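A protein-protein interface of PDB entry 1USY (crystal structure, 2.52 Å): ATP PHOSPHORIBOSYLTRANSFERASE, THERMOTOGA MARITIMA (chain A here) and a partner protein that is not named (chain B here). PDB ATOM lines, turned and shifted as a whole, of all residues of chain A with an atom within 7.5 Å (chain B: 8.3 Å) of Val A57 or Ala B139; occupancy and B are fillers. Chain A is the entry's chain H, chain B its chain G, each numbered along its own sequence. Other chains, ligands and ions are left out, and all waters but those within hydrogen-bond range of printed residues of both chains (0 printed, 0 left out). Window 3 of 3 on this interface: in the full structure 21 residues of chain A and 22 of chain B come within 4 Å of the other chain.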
ATOM      1  N   LEU A   2     -32.335  29.949  29.976  1.00  0.00           N
ATOM      2  CA  LEU A   2     -30.907  30.198  29.997  1.00  0.00           C
ATOM      3  C   LEU A   2     -30.220  28.868  30.079  1.00  0.00           C
ATOM      4  O   LEU A   2     -30.561  28.067  30.948  1.00  0.00           O
ATOM      5  CB  LEU A   2     -30.547  30.968  31.243  1.00  0.00           C
ATOM      6  CG  LEU A   2     -29.798  32.289  31.196  1.00  0.00           C
ATOM      7  CD1 LEU A   2     -30.196  33.156  30.005  1.00  0.00           C
ATOM      8  CD2 LEU A   2     -30.103  33.028  32.518  1.00  0.00           C
ATOM      9  N   LYS A   3     -29.251  28.639  29.204  1.00  0.00           N
ATOM     10  CA  LYS A   3     -28.416  27.428  29.258  1.00  0.00           C
ATOM     11  C   LYS A   3     -27.035  27.725  29.832  1.00  0.00           C
ATOM     12  O   LYS A   3     -26.350  28.676  29.389  1.00  0.00           O
ATOM     13  CB  LYS A   3     -28.276  26.802  27.881  1.00  0.00           C
ATOM     14  CG  LYS A   3     -29.632  26.596  27.186  1.00  0.00           C
ATOM     15  CD  LYS A   3     -29.490  26.102  25.748  1.00  0.00           C
ATOM     16  CE  LYS A   3     -30.258  27.014  24.786  1.00  0.00           C
ATOM     17  NZ  LYS A   3     -30.416  26.466  23.383  1.00  0.00           N
ATOM     18  N   LEU A   4     -26.658  26.930  30.832  1.00  0.00           N
ATOM     19  CA  LEU A   4     -25.376  27.075  31.499  1.00  0.00           C
ATOM     20  C   LEU A   4     -24.460  25.878  31.309  1.00  0.00           C
ATOM     21  O   LEU A   4     -24.883  24.694  31.455  1.00  0.00           O
ATOM     22  CB  LEU A   4     -25.517  27.265  33.008  1.00  0.00           C
ATOM     23  CG  LEU A   4     -26.496  28.188  33.679  1.00  0.00           C
ATOM     24  CD1 LEU A   4     -26.015  28.323  35.098  1.00  0.00           C
ATOM     25  CD2 LEU A   4     -26.655  29.521  33.006  1.00  0.00           C
ATOM     26  N   ALA A   5     -23.198  26.189  31.022  1.00  0.00           N
ATOM     27  CA  ALA A   5     -22.182  25.162  30.878  1.00  0.00           C
ATOM     28  C   ALA A   5     -21.417  25.126  32.214  1.00  0.00           C
ATOM     29  O   ALA A   5     -20.734  26.109  32.617  1.00  0.00           O
ATOM     30  CB  ALA A   5     -21.271  25.458  29.690  1.00  0.00           C
ATOM     31  N   LEU A  33     -26.735  16.097  32.355  1.00  0.00           N
ATOM     32  CA  LEU A  33     -27.679  17.144  31.965  1.00  0.00           C
ATOM     33  C   LEU A  33     -28.705  17.405  33.063  1.00  0.00           C
ATOM     34  O   LEU A  33     -29.252  16.455  33.658  1.00  0.00           O
ATOM     35  CB  LEU A  33     -28.378  16.738  30.671  1.00  0.00           C
ATOM     36  CG  LEU A  33     -29.529  17.566  30.114  1.00  0.00           C
ATOM     37  CD1 LEU A  33     -29.007  18.736  29.356  1.00  0.00           C
ATOM     38  CD2 LEU A  33     -30.336  16.639  29.189  1.00  0.00           C
ATOM     39  N   VAL A  40     -31.374  25.188  32.048  1.00  0.00           N
ATOM     40  CA  VAL A  40     -30.845  23.845  31.857  1.00  0.00           C
ATOM     41  C   VAL A  40     -29.342  23.897  31.928  1.00  0.00           C
ATOM     42  O   VAL A  40     -28.742  24.760  31.322  1.00  0.00           O
ATOM     43  CB  VAL A  40     -31.317  23.134  30.505  1.00  0.00           C
ATOM     44  CG1 VAL A  40     -32.842  23.117  30.393  1.00  0.00           C
ATOM     45  CG2 VAL A  40     -30.702  23.774  29.286  1.00  0.00           C
ATOM     46  N   PHE A  42     -25.637  22.062  31.176  1.00  0.00           N
ATOM     47  CA  PHE A  42     -24.762  21.059  30.642  1.00  0.00           C
ATOM     48  C   PHE A  42     -23.609  20.863  31.596  1.00  0.00           C
ATOM     49  O   PHE A  42     -22.918  21.801  31.952  1.00  0.00           O
ATOM     50  CB  PHE A  42     -24.284  21.478  29.256  1.00  0.00           C
ATOM     51  CG  PHE A  42     -25.407  21.831  28.314  1.00  0.00           C
ATOM     52  CD1 PHE A  42     -25.452  23.097  27.708  1.00  0.00           C
ATOM     53  CD2 PHE A  42     -26.440  20.901  28.030  1.00  0.00           C
ATOM     54  CE1 PHE A  42     -26.501  23.436  26.815  1.00  0.00           C
ATOM     55  CE2 PHE A  42     -27.478  21.226  27.145  1.00  0.00           C
ATOM     56  CZ  PHE A  42     -27.517  22.510  26.542  1.00  0.00           C
ATOM     57  N   VAL A  49     -15.886  24.360  28.498  1.00  0.00           N
ATOM     58  CA  VAL A  49     -16.825  25.441  28.744  1.00  0.00           C
ATOM     59  C   VAL A  49     -16.800  26.467  27.635  1.00  0.00           C
ATOM     60  O   VAL A  49     -17.848  26.771  27.060  1.00  0.00           O
ATOM     61  CB  VAL A  49     -16.576  26.136  30.081  1.00  0.00           C
ATOM     62  CG1 VAL A  49     -17.047  27.590  30.003  1.00  0.00           C
ATOM     63  CG2 VAL A  49     -17.270  25.385  31.187  1.00  0.00           C
ATOM     64  N   THR A  51     -15.867  26.276  24.649  1.00  0.00           N
ATOM     65  CA  THR A  51     -16.376  25.836  23.369  1.00  0.00           C
ATOM     66  C   THR A  51     -17.891  25.667  23.342  1.00  0.00           C
ATOM     67  O   THR A  51     -18.466  25.610  22.299  1.00  0.00           O
ATOM     68  CB  THR A  51     -15.578  24.635  22.757  1.00  0.00           C
ATOM     69  OG1 THR A  51     -16.346  23.429  22.806  1.00  0.00           O
ATOM     70  CG2 THR A  51     -14.325  24.323  23.574  1.00  0.00           C
ATOM     71  N   TYR A  52     -18.537  25.662  24.490  1.00  0.00           N
ATOM     72  CA  TYR A  52     -19.993  25.723  24.526  1.00  0.00           C
ATOM     73  C   TYR A  52     -20.487  27.166  24.390  1.00  0.00           C
ATOM     74  O   TYR A  52     -21.598  27.413  23.911  1.00  0.00           O
ATOM     75  CB  TYR A  52     -20.510  25.109  25.830  1.00  0.00           C
ATOM     76  CG  TYR A  52     -20.783  23.619  25.709  1.00  0.00           C
ATOM     77  CD1 TYR A  52     -19.734  22.700  25.727  1.00  0.00           C
ATOM     78  CD2 TYR A  52     -22.094  23.129  25.564  1.00  0.00           C
ATOM     79  CE1 TYR A  52     -19.963  21.365  25.619  1.00  0.00           C
ATOM     80  CE2 TYR A  52     -22.340  21.770  25.453  1.00  0.00           C
ATOM     81  CZ  TYR A  52     -21.255  20.892  25.493  1.00  0.00           C
ATOM     82  OH  TYR A  52     -21.418  19.541  25.348  1.00  0.00           O
ATOM     83  N   LEU A  53     -19.643  28.114  24.792  1.00  0.00           N
ATOM     84  CA  LEU A  53     -20.018  29.509  24.862  1.00  0.00           C
ATOM     85  C   LEU A  53     -19.761  30.249  23.569  1.00  0.00           C
ATOM     86  O   LEU A  53     -20.541  31.142  23.201  1.00  0.00           O
ATOM     87  CB  LEU A  53     -19.282  30.153  26.039  1.00  0.00           C
ATOM     88  CG  LEU A  53     -19.884  29.682  27.381  1.00  0.00           C
ATOM     89  CD1 LEU A  53     -18.953  29.961  28.506  1.00  0.00           C
ATOM     90  CD2 LEU A  53     -21.172  30.364  27.635  1.00  0.00           C
ATOM     91  N   VAL A  54     -18.666  29.877  22.891  1.00  0.00           N
ATOM     92  CA  VAL A  54     -18.307  30.431  21.565  1.00  0.00           C
ATOM     93  C   VAL A  54     -19.351  30.090  20.496  1.00  0.00           C
ATOM     94  O   VAL A  54     -19.689  30.926  19.661  1.00  0.00           O
ATOM     95  CB  VAL A  54     -16.834  30.024  21.085  1.00  0.00           C
ATOM     96  CG1 VAL A  54     -16.562  30.485  19.678  1.00  0.00           C
ATOM     97  CG2 VAL A  54     -15.763  30.671  21.987  1.00  0.00           C
ATOM     98  N   HIS A  55     -19.856  28.861  20.511  1.00  0.00           N
ATOM     99  CA  HIS A  55     -20.842  28.488  19.514  1.00  0.00           C
ATOM    100  C   HIS A  55     -22.238  28.909  19.976  1.00  0.00           C
ATOM    101  O   HIS A  55     -23.230  28.565  19.363  1.00  0.00           O
ATOM    102  CB  HIS A  55     -20.766  26.994  19.129  1.00  0.00           C
ATOM    103  CG  HIS A  55     -21.334  26.698  17.758  1.00  0.00           C
ATOM    104  ND1 HIS A  55     -22.679  26.826  17.458  1.00  0.00           N
ATOM    105  CD2 HIS A  55     -20.731  26.309  16.605  1.00  0.00           C
ATOM    106  CE1 HIS A  55     -22.877  26.530  16.185  1.00  0.00           C
ATOM    107  NE2 HIS A  55     -21.713  26.207  15.646  1.00  0.00           N
ATOM    108  N   GLY A  56     -22.316  29.670  21.055  1.00  0.00           N
ATOM    109  CA  GLY A  56     -23.616  30.054  21.547  1.00  0.00           C
ATOM    110  C   GLY A  56     -24.584  28.901  21.820  1.00  0.00           C
ATOM    111  O   GLY A  56     -25.811  29.105  21.700  1.00  0.00           O
ATOM    112  N   VAL A  57     -24.074  27.708  22.188  1.00  0.00           N
ATOM    113  CA  VAL A  57     -24.970  26.635  22.656  1.00  0.00           C
ATOM    114  C   VAL A  57     -25.256  26.723  24.161  1.00  0.00           C
ATOM    115  O   VAL A  57     -26.180  26.112  24.668  1.00  0.00           O
ATOM    116  CB  VAL A  57     -24.552  25.214  22.198  1.00  0.00           C
ATOM    117  CG1 VAL A  57     -24.239  25.212  20.706  1.00  0.00           C
ATOM    118  CG2 VAL A  57     -23.407  24.690  22.964  1.00  0.00           C
ATOM    119  N   ALA A  58     -24.442  27.487  24.863  1.00  0.00           N
ATOM    120  CA  ALA A  58     -24.739  27.904  26.225  1.00  0.00           C
ATOM    121  C   ALA A  58     -24.551  29.411  26.319  1.00  0.00           C
ATOM    122  O   ALA A  58     -23.760  29.996  25.579  1.00  0.00           O
ATOM    123  CB  ALA A  58     -23.831  27.228  27.231  1.00  0.00           C
ATOM    124  N   ASP A  59     -25.246  29.995  27.274  1.00  0.00           N
ATOM    125  CA  ASP A  59     -25.268  31.421  27.502  1.00  0.00           C
ATOM    126  C   ASP A  59     -24.290  31.851  28.596  1.00  0.00           C
ATOM    127  O   ASP A  59     -23.649  32.899  28.507  1.00  0.00           O
ATOM    128  CB  ASP A  59     -26.702  31.801  27.859  1.00  0.00           C
ATOM    129  CG  ASP A  59     -27.700  31.362  26.766  1.00  0.00           C
ATOM    130  OD1 ASP A  59     -27.435  31.596  25.563  1.00  0.00           O
ATOM    131  OD2 ASP A  59     -28.752  30.735  27.001  1.00  0.00           O
ATOM    132  N   ILE A  60     -24.124  31.017  29.603  1.00  0.00           N
ATOM    133  CA  ILE A  60     -23.309  31.359  30.749  1.00  0.00           C
ATOM    134  C   ILE A  60     -22.501  30.123  31.159  1.00  0.00           C
ATOM    135  O   ILE A  60     -22.956  28.987  31.017  1.00  0.00           O
ATOM    136  CB  ILE A  60     -24.192  31.832  31.909  1.00  0.00           C
ATOM    137  CG1 ILE A  60     -24.869  33.160  31.525  1.00  0.00           C
ATOM    138  CG2 ILE A  60     -23.345  31.965  33.174  1.00  0.00           C
ATOM    139  CD1 ILE A  60     -25.966  33.648  32.446  1.00  0.00           C
ATOM    140  N   ASN A 176     -21.905  34.341  26.979  1.00  0.00           N
ATOM    141  CA  ASN A 176     -21.792  34.496  25.545  1.00  0.00           C
ATOM    142  C   ASN A 176     -22.043  36.002  25.221  1.00  0.00           C
ATOM    143  O   ASN A 176     -23.018  36.610  25.708  1.00  0.00           O
ATOM    144  CB  ASN A 176     -22.788  33.614  24.780  1.00  0.00           C
ATOM    145  CG  ASN A 176     -22.759  33.906  23.284  1.00  0.00           C
ATOM    146  OD1 ASN A 176     -21.802  33.557  22.577  1.00  0.00           O
ATOM    147  ND2 ASN A 176     -23.761  34.610  22.811  1.00  0.00           N
ATOM    148  N   SER A 179     -25.599  36.621  23.795  1.00  0.00           N
ATOM    149  CA  SER A 179     -26.726  36.220  24.640  1.00  0.00           C
ATOM    150  C   SER A 179     -27.061  37.330  25.638  1.00  0.00           C
ATOM    151  O   SER A 179     -28.201  37.510  26.104  1.00  0.00           O
ATOM    152  CB  SER A 179     -26.375  34.960  25.396  1.00  0.00           C
ATOM    153  OG  SER A 179     -26.083  33.916  24.498  1.00  0.00           O
ATOM    154  N   LYS A 183     -30.672  38.270  25.179  1.00  0.00           N
ATOM    155  CA  LYS A 183     -31.599  37.868  26.220  1.00  0.00           C
ATOM    156  C   LYS A 183     -31.080  38.440  27.532  1.00  0.00           C
ATOM    157  O   LYS A 183     -30.903  37.723  28.542  1.00  0.00           O
ATOM    158  CB  LYS A 183     -31.735  36.340  26.270  1.00  0.00           C
ATOM    159  CG  LYS A 183     -30.459  35.587  26.373  1.00  0.00           C
ATOM    160  CD  LYS A 183     -30.710  34.088  26.281  1.00  0.00           C
ATOM    161  CE  LYS A 183     -30.416  33.497  24.891  1.00  0.00           C
ATOM    162  NZ  LYS A 183     -30.494  31.981  24.916  1.00  0.00           N
ATOM    163  N   ARG B 104     -21.133  17.475  11.582  1.00  0.00           N
ATOM    164  CA  ARG B 104     -20.394  17.893  12.777  1.00  0.00           C
ATOM    165  C   ARG B 104     -20.318  16.748  13.765  1.00  0.00           C
ATOM    166  O   ARG B 104     -21.370  16.254  14.200  1.00  0.00           O
ATOM    167  CB  ARG B 104     -21.075  19.078  13.467  1.00  0.00           C
ATOM    168  CG  ARG B 104     -20.904  20.432  12.804  1.00  0.00           C
ATOM    169  CD  ARG B 104     -21.736  21.509  13.458  1.00  0.00           C
ATOM    170  NE  ARG B 104     -23.166  21.325  13.193  1.00  0.00           N
ATOM    171  CZ  ARG B 104     -24.154  21.521  14.085  1.00  0.00           C
ATOM    172  NH1 ARG B 104     -23.892  21.909  15.335  1.00  0.00           N
ATOM    173  NH2 ARG B 104     -25.424  21.324  13.724  1.00  0.00           N
ATOM    174  N   ILE B 127     -15.139  18.312  16.465  1.00  0.00           N
ATOM    175  CA  ILE B 127     -15.126  19.078  17.700  1.00  0.00           C
ATOM    176  C   ILE B 127     -14.623  18.201  18.835  1.00  0.00           C
ATOM    177  O   ILE B 127     -15.348  17.344  19.354  1.00  0.00           O
ATOM    178  CB  ILE B 127     -16.521  19.528  18.021  1.00  0.00           C
ATOM    179  CG1 ILE B 127     -17.137  20.197  16.786  1.00  0.00           C
ATOM    180  CG2 ILE B 127     -16.499  20.460  19.251  1.00  0.00           C
ATOM    181  CD1 ILE B 127     -18.499  20.638  17.000  1.00  0.00           C
ATOM    182  N   SER B 132     -18.164  14.079  28.591  1.00  0.00           N
ATOM    183  CA  SER B 132     -19.603  14.432  28.500  1.00  0.00           C
ATOM    184  C   SER B 132     -20.100  14.519  27.052  1.00  0.00           C
ATOM    185  O   SER B 132     -21.087  15.184  26.733  1.00  0.00           O
ATOM    186  CB  SER B 132     -19.926  15.701  29.304  1.00  0.00           C
ATOM    187  OG  SER B 132     -19.332  15.649  30.585  1.00  0.00           O
ATOM    188  N   VAL B 133     -19.408  13.791  26.209  1.00  0.00           N
ATOM    189  CA  VAL B 133     -19.608  13.756  24.787  1.00  0.00           C
ATOM    190  C   VAL B 133     -21.039  13.546  24.303  1.00  0.00           C
ATOM    191  O   VAL B 133     -21.338  13.934  23.196  1.00  0.00           O
ATOM    192  CB  VAL B 133     -18.714  12.671  24.240  1.00  0.00           C
ATOM    193  CG1 VAL B 133     -18.859  12.499  22.738  1.00  0.00           C
ATOM    194  CG2 VAL B 133     -17.271  12.985  24.606  1.00  0.00           C
ATOM    195  N   GLU B 134     -21.905  12.953  25.129  1.00  0.00           N
ATOM    196  CA  GLU B 134     -23.269  12.539  24.727  1.00  0.00           C
ATOM    197  C   GLU B 134     -24.222  13.681  24.671  1.00  0.00           C
ATOM    198  O   GLU B 134     -25.342  13.512  24.202  1.00  0.00           O
ATOM    199  CB  GLU B 134     -23.857  11.534  25.714  1.00  0.00           C
ATOM    200  CG  GLU B 134     -23.583  10.085  25.369  1.00  0.00           C
ATOM    201  CD  GLU B 134     -22.152   9.687  25.671  1.00  0.00           C
ATOM    202  OE1 GLU B 134     -21.416  10.477  26.342  1.00  0.00           O
ATOM    203  OE2 GLU B 134     -21.775   8.579  25.271  1.00  0.00           O
ATOM    204  N   LEU B 135     -23.802  14.806  25.254  1.00  0.00           N
ATOM    205  CA  LEU B 135     -24.416  16.118  25.083  1.00  0.00           C
ATOM    206  C   LEU B 135     -23.834  16.515  23.786  1.00  0.00           C
ATOM    207  O   LEU B 135     -22.902  15.872  23.311  1.00  0.00           O
ATOM    208  CB  LEU B 135     -23.835  17.090  26.076  1.00  0.00           C
ATOM    209  CG  LEU B 135     -24.087  16.897  27.546  1.00  0.00           C
ATOM    210  CD1 LEU B 135     -23.166  17.798  28.272  1.00  0.00           C
ATOM    211  CD2 LEU B 135     -25.513  17.235  27.849  1.00  0.00           C
ATOM    212  N   ALA B 136     -24.293  17.583  23.187  1.00  0.00           N
ATOM    213  CA  ALA B 136     -23.624  17.974  21.939  1.00  0.00           C
ATOM    214  C   ALA B 136     -24.548  17.784  20.802  1.00  0.00           C
ATOM    215  O   ALA B 136     -24.830  18.749  20.141  1.00  0.00           O
ATOM    216  CB  ALA B 136     -22.313  17.214  21.698  1.00  0.00           C
ATOM    217  N   PRO B 137     -25.044  16.583  20.547  1.00  0.00           N
ATOM    218  CA  PRO B 137     -26.271  16.473  19.742  1.00  0.00           C
ATOM    219  C   PRO B 137     -27.441  17.152  20.434  1.00  0.00           C
ATOM    220  O   PRO B 137     -28.200  17.816  19.784  1.00  0.00           O
ATOM    221  CB  PRO B 137     -26.465  14.968  19.574  1.00  0.00           C
ATOM    222  CG  PRO B 137     -25.103  14.324  19.949  1.00  0.00           C
ATOM    223  CD  PRO B 137     -24.463  15.272  20.890  1.00  0.00           C
ATOM    224  N   ILE B 138     -27.539  17.038  21.752  1.00  0.00           N
ATOM    225  CA  ILE B 138     -28.587  17.705  22.531  1.00  0.00           C
ATOM    226  C   ILE B 138     -28.385  19.189  22.566  1.00  0.00           C
ATOM    227  O   ILE B 138     -29.334  19.948  22.439  1.00  0.00           O
ATOM    228  CB  ILE B 138     -28.604  17.248  24.012  1.00  0.00           C
ATOM    229  CG1 ILE B 138     -28.062  15.809  24.233  1.00  0.00           C
ATOM    230  CG2 ILE B 138     -30.004  17.463  24.593  1.00  0.00           C
ATOM    231  CD1 ILE B 138     -28.350  14.739  23.151  1.00  0.00           C
ATOM    232  N   ALA B 139     -27.154  19.601  22.801  1.00  0.00           N
ATOM    233  CA  ALA B 139     -26.840  21.020  22.903  1.00  0.00           C
ATOM    234  C   ALA B 139     -26.845  21.701  21.546  1.00  0.00           C
ATOM    235  O   ALA B 139     -27.092  22.882  21.470  1.00  0.00           O
ATOM    236  CB  ALA B 139     -25.470  21.209  23.583  1.00  0.00           C
ATOM    237  N   GLY B 140     -26.550  20.960  20.480  1.00  0.00           N
ATOM    238  CA  GLY B 140     -26.408  21.555  19.175  1.00  0.00           C
ATOM    239  C   GLY B 140     -24.985  21.868  18.816  1.00  0.00           C
ATOM    240  O   GLY B 140     -24.740  22.587  17.846  1.00  0.00           O
ATOM    241  N   LEU B 141     -24.046  21.338  19.592  1.00  0.00           N
ATOM    242  CA  LEU B 141     -22.633  21.442  19.275  1.00  0.00           C
ATOM    243  C   LEU B 141     -22.269  20.536  18.102  1.00  0.00           C
ATOM    244  O   LEU B 141     -21.311  20.779  17.379  1.00  0.00           O
ATOM    245  CB  LEU B 141     -21.809  21.067  20.494  1.00  0.00           C
ATOM    246  CG  LEU B 141     -20.679  21.966  20.970  1.00  0.00           C
ATOM    247  CD1 LEU B 141     -19.470  21.106  20.960  1.00  0.00           C
ATOM    248  CD2 LEU B 141     -20.454  23.259  20.145  1.00  0.00           C
ATOM    249  N   SER B 142     -23.020  19.471  17.904  1.00  0.00           N
ATOM    250  CA  SER B 142     -22.643  18.530  16.863  1.00  0.00           C
ATOM    251  C   SER B 142     -23.861  17.821  16.364  1.00  0.00           C
ATOM    252  O   SER B 142     -24.879  17.833  17.027  1.00  0.00           O
ATOM    253  CB  SER B 142     -21.538  17.563  17.342  1.00  0.00           C
ATOM    254  OG  SER B 142     -22.066  16.401  17.927  1.00  0.00           O
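The backbone NH of Leu B141 sits at hydrogen-bond distance from the backbone carbonyl oxygen of Ala B136, at 2.8 Å. O of Gly B140 sits at hydrogen-bond distance from NH1 of Arg B104, 2.7 Å away. The backbone carbonyl oxygen (O) of Tyr A52 is in hydrogen-bond range of the backbone NH (N) of Ala A58 (3.0 Å). The backbone NH of Val A57 is in hydrogen-bond range of the backbone carbonyl oxygen of Tyr A52 (3.0 Å). NH1 of Arg B104 is in hydrogen-bond range of O of Leu B141, at 3.5 Å. O of Leu A4 lies within hydrogen-bond range of N of Phe A42, at 2.8 Å.
CD2 of Leu B135 touches CD2 of Phe A42, 3.8 Å away. Phe A42 touches Ala B139 (CZ to CB, 3.8 Å). CD2 of Leu B141 touches O of Thr A51 (3.8 Å). OH of Tyr A52 touches CB of Leu B135 (3.5 Å). Ala B139 touches Tyr A52 (CB to CE2, 3.7 Å). His A55 touches Leu B141. O of Ala B139 touches CB of Val A57, at 3.5 Å. Val A57 touches Gly B140.
Leu A4 touches none of the printed residues of chain B. Printed residues of chain B within 4 Å of Phe A42: Leu B135 (3.8 Å) and Ala B139 (3.8 Å). Printed residues of chain B within 4 Å of Tyr A52: Leu B135 (3.5 Å) and Ala B139 (3.7 Å). Printed residues of chain B within 4 Å of His A55: Leu B141. No residue of chain B comes within 4 Å of Gly A56. Val A57 touches two residues of chain B. No residue of chain B comes within 4 Å of Ala A58. Of chain A, only Phe A42, Tyr A52 and Val A57 come within 4 Å of Ala B139. Of the printed residues of chain A, Gly B140 touches Val A57. Printed residues of chain A within 4 Å of Leu B141: Thr A51 and His A55. The nearest residue of chain B that does not touch Val A57 is Leu B141 (4.04 Å). The nearest printed residue of chain A that does not touch Leu B135 is Leu A33 (4.1 Å).
Among the printed residues, no Asp or Glu carboxylate lies within 4 Å of a Lys or Arg side-chain nitrogen of the other chain.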
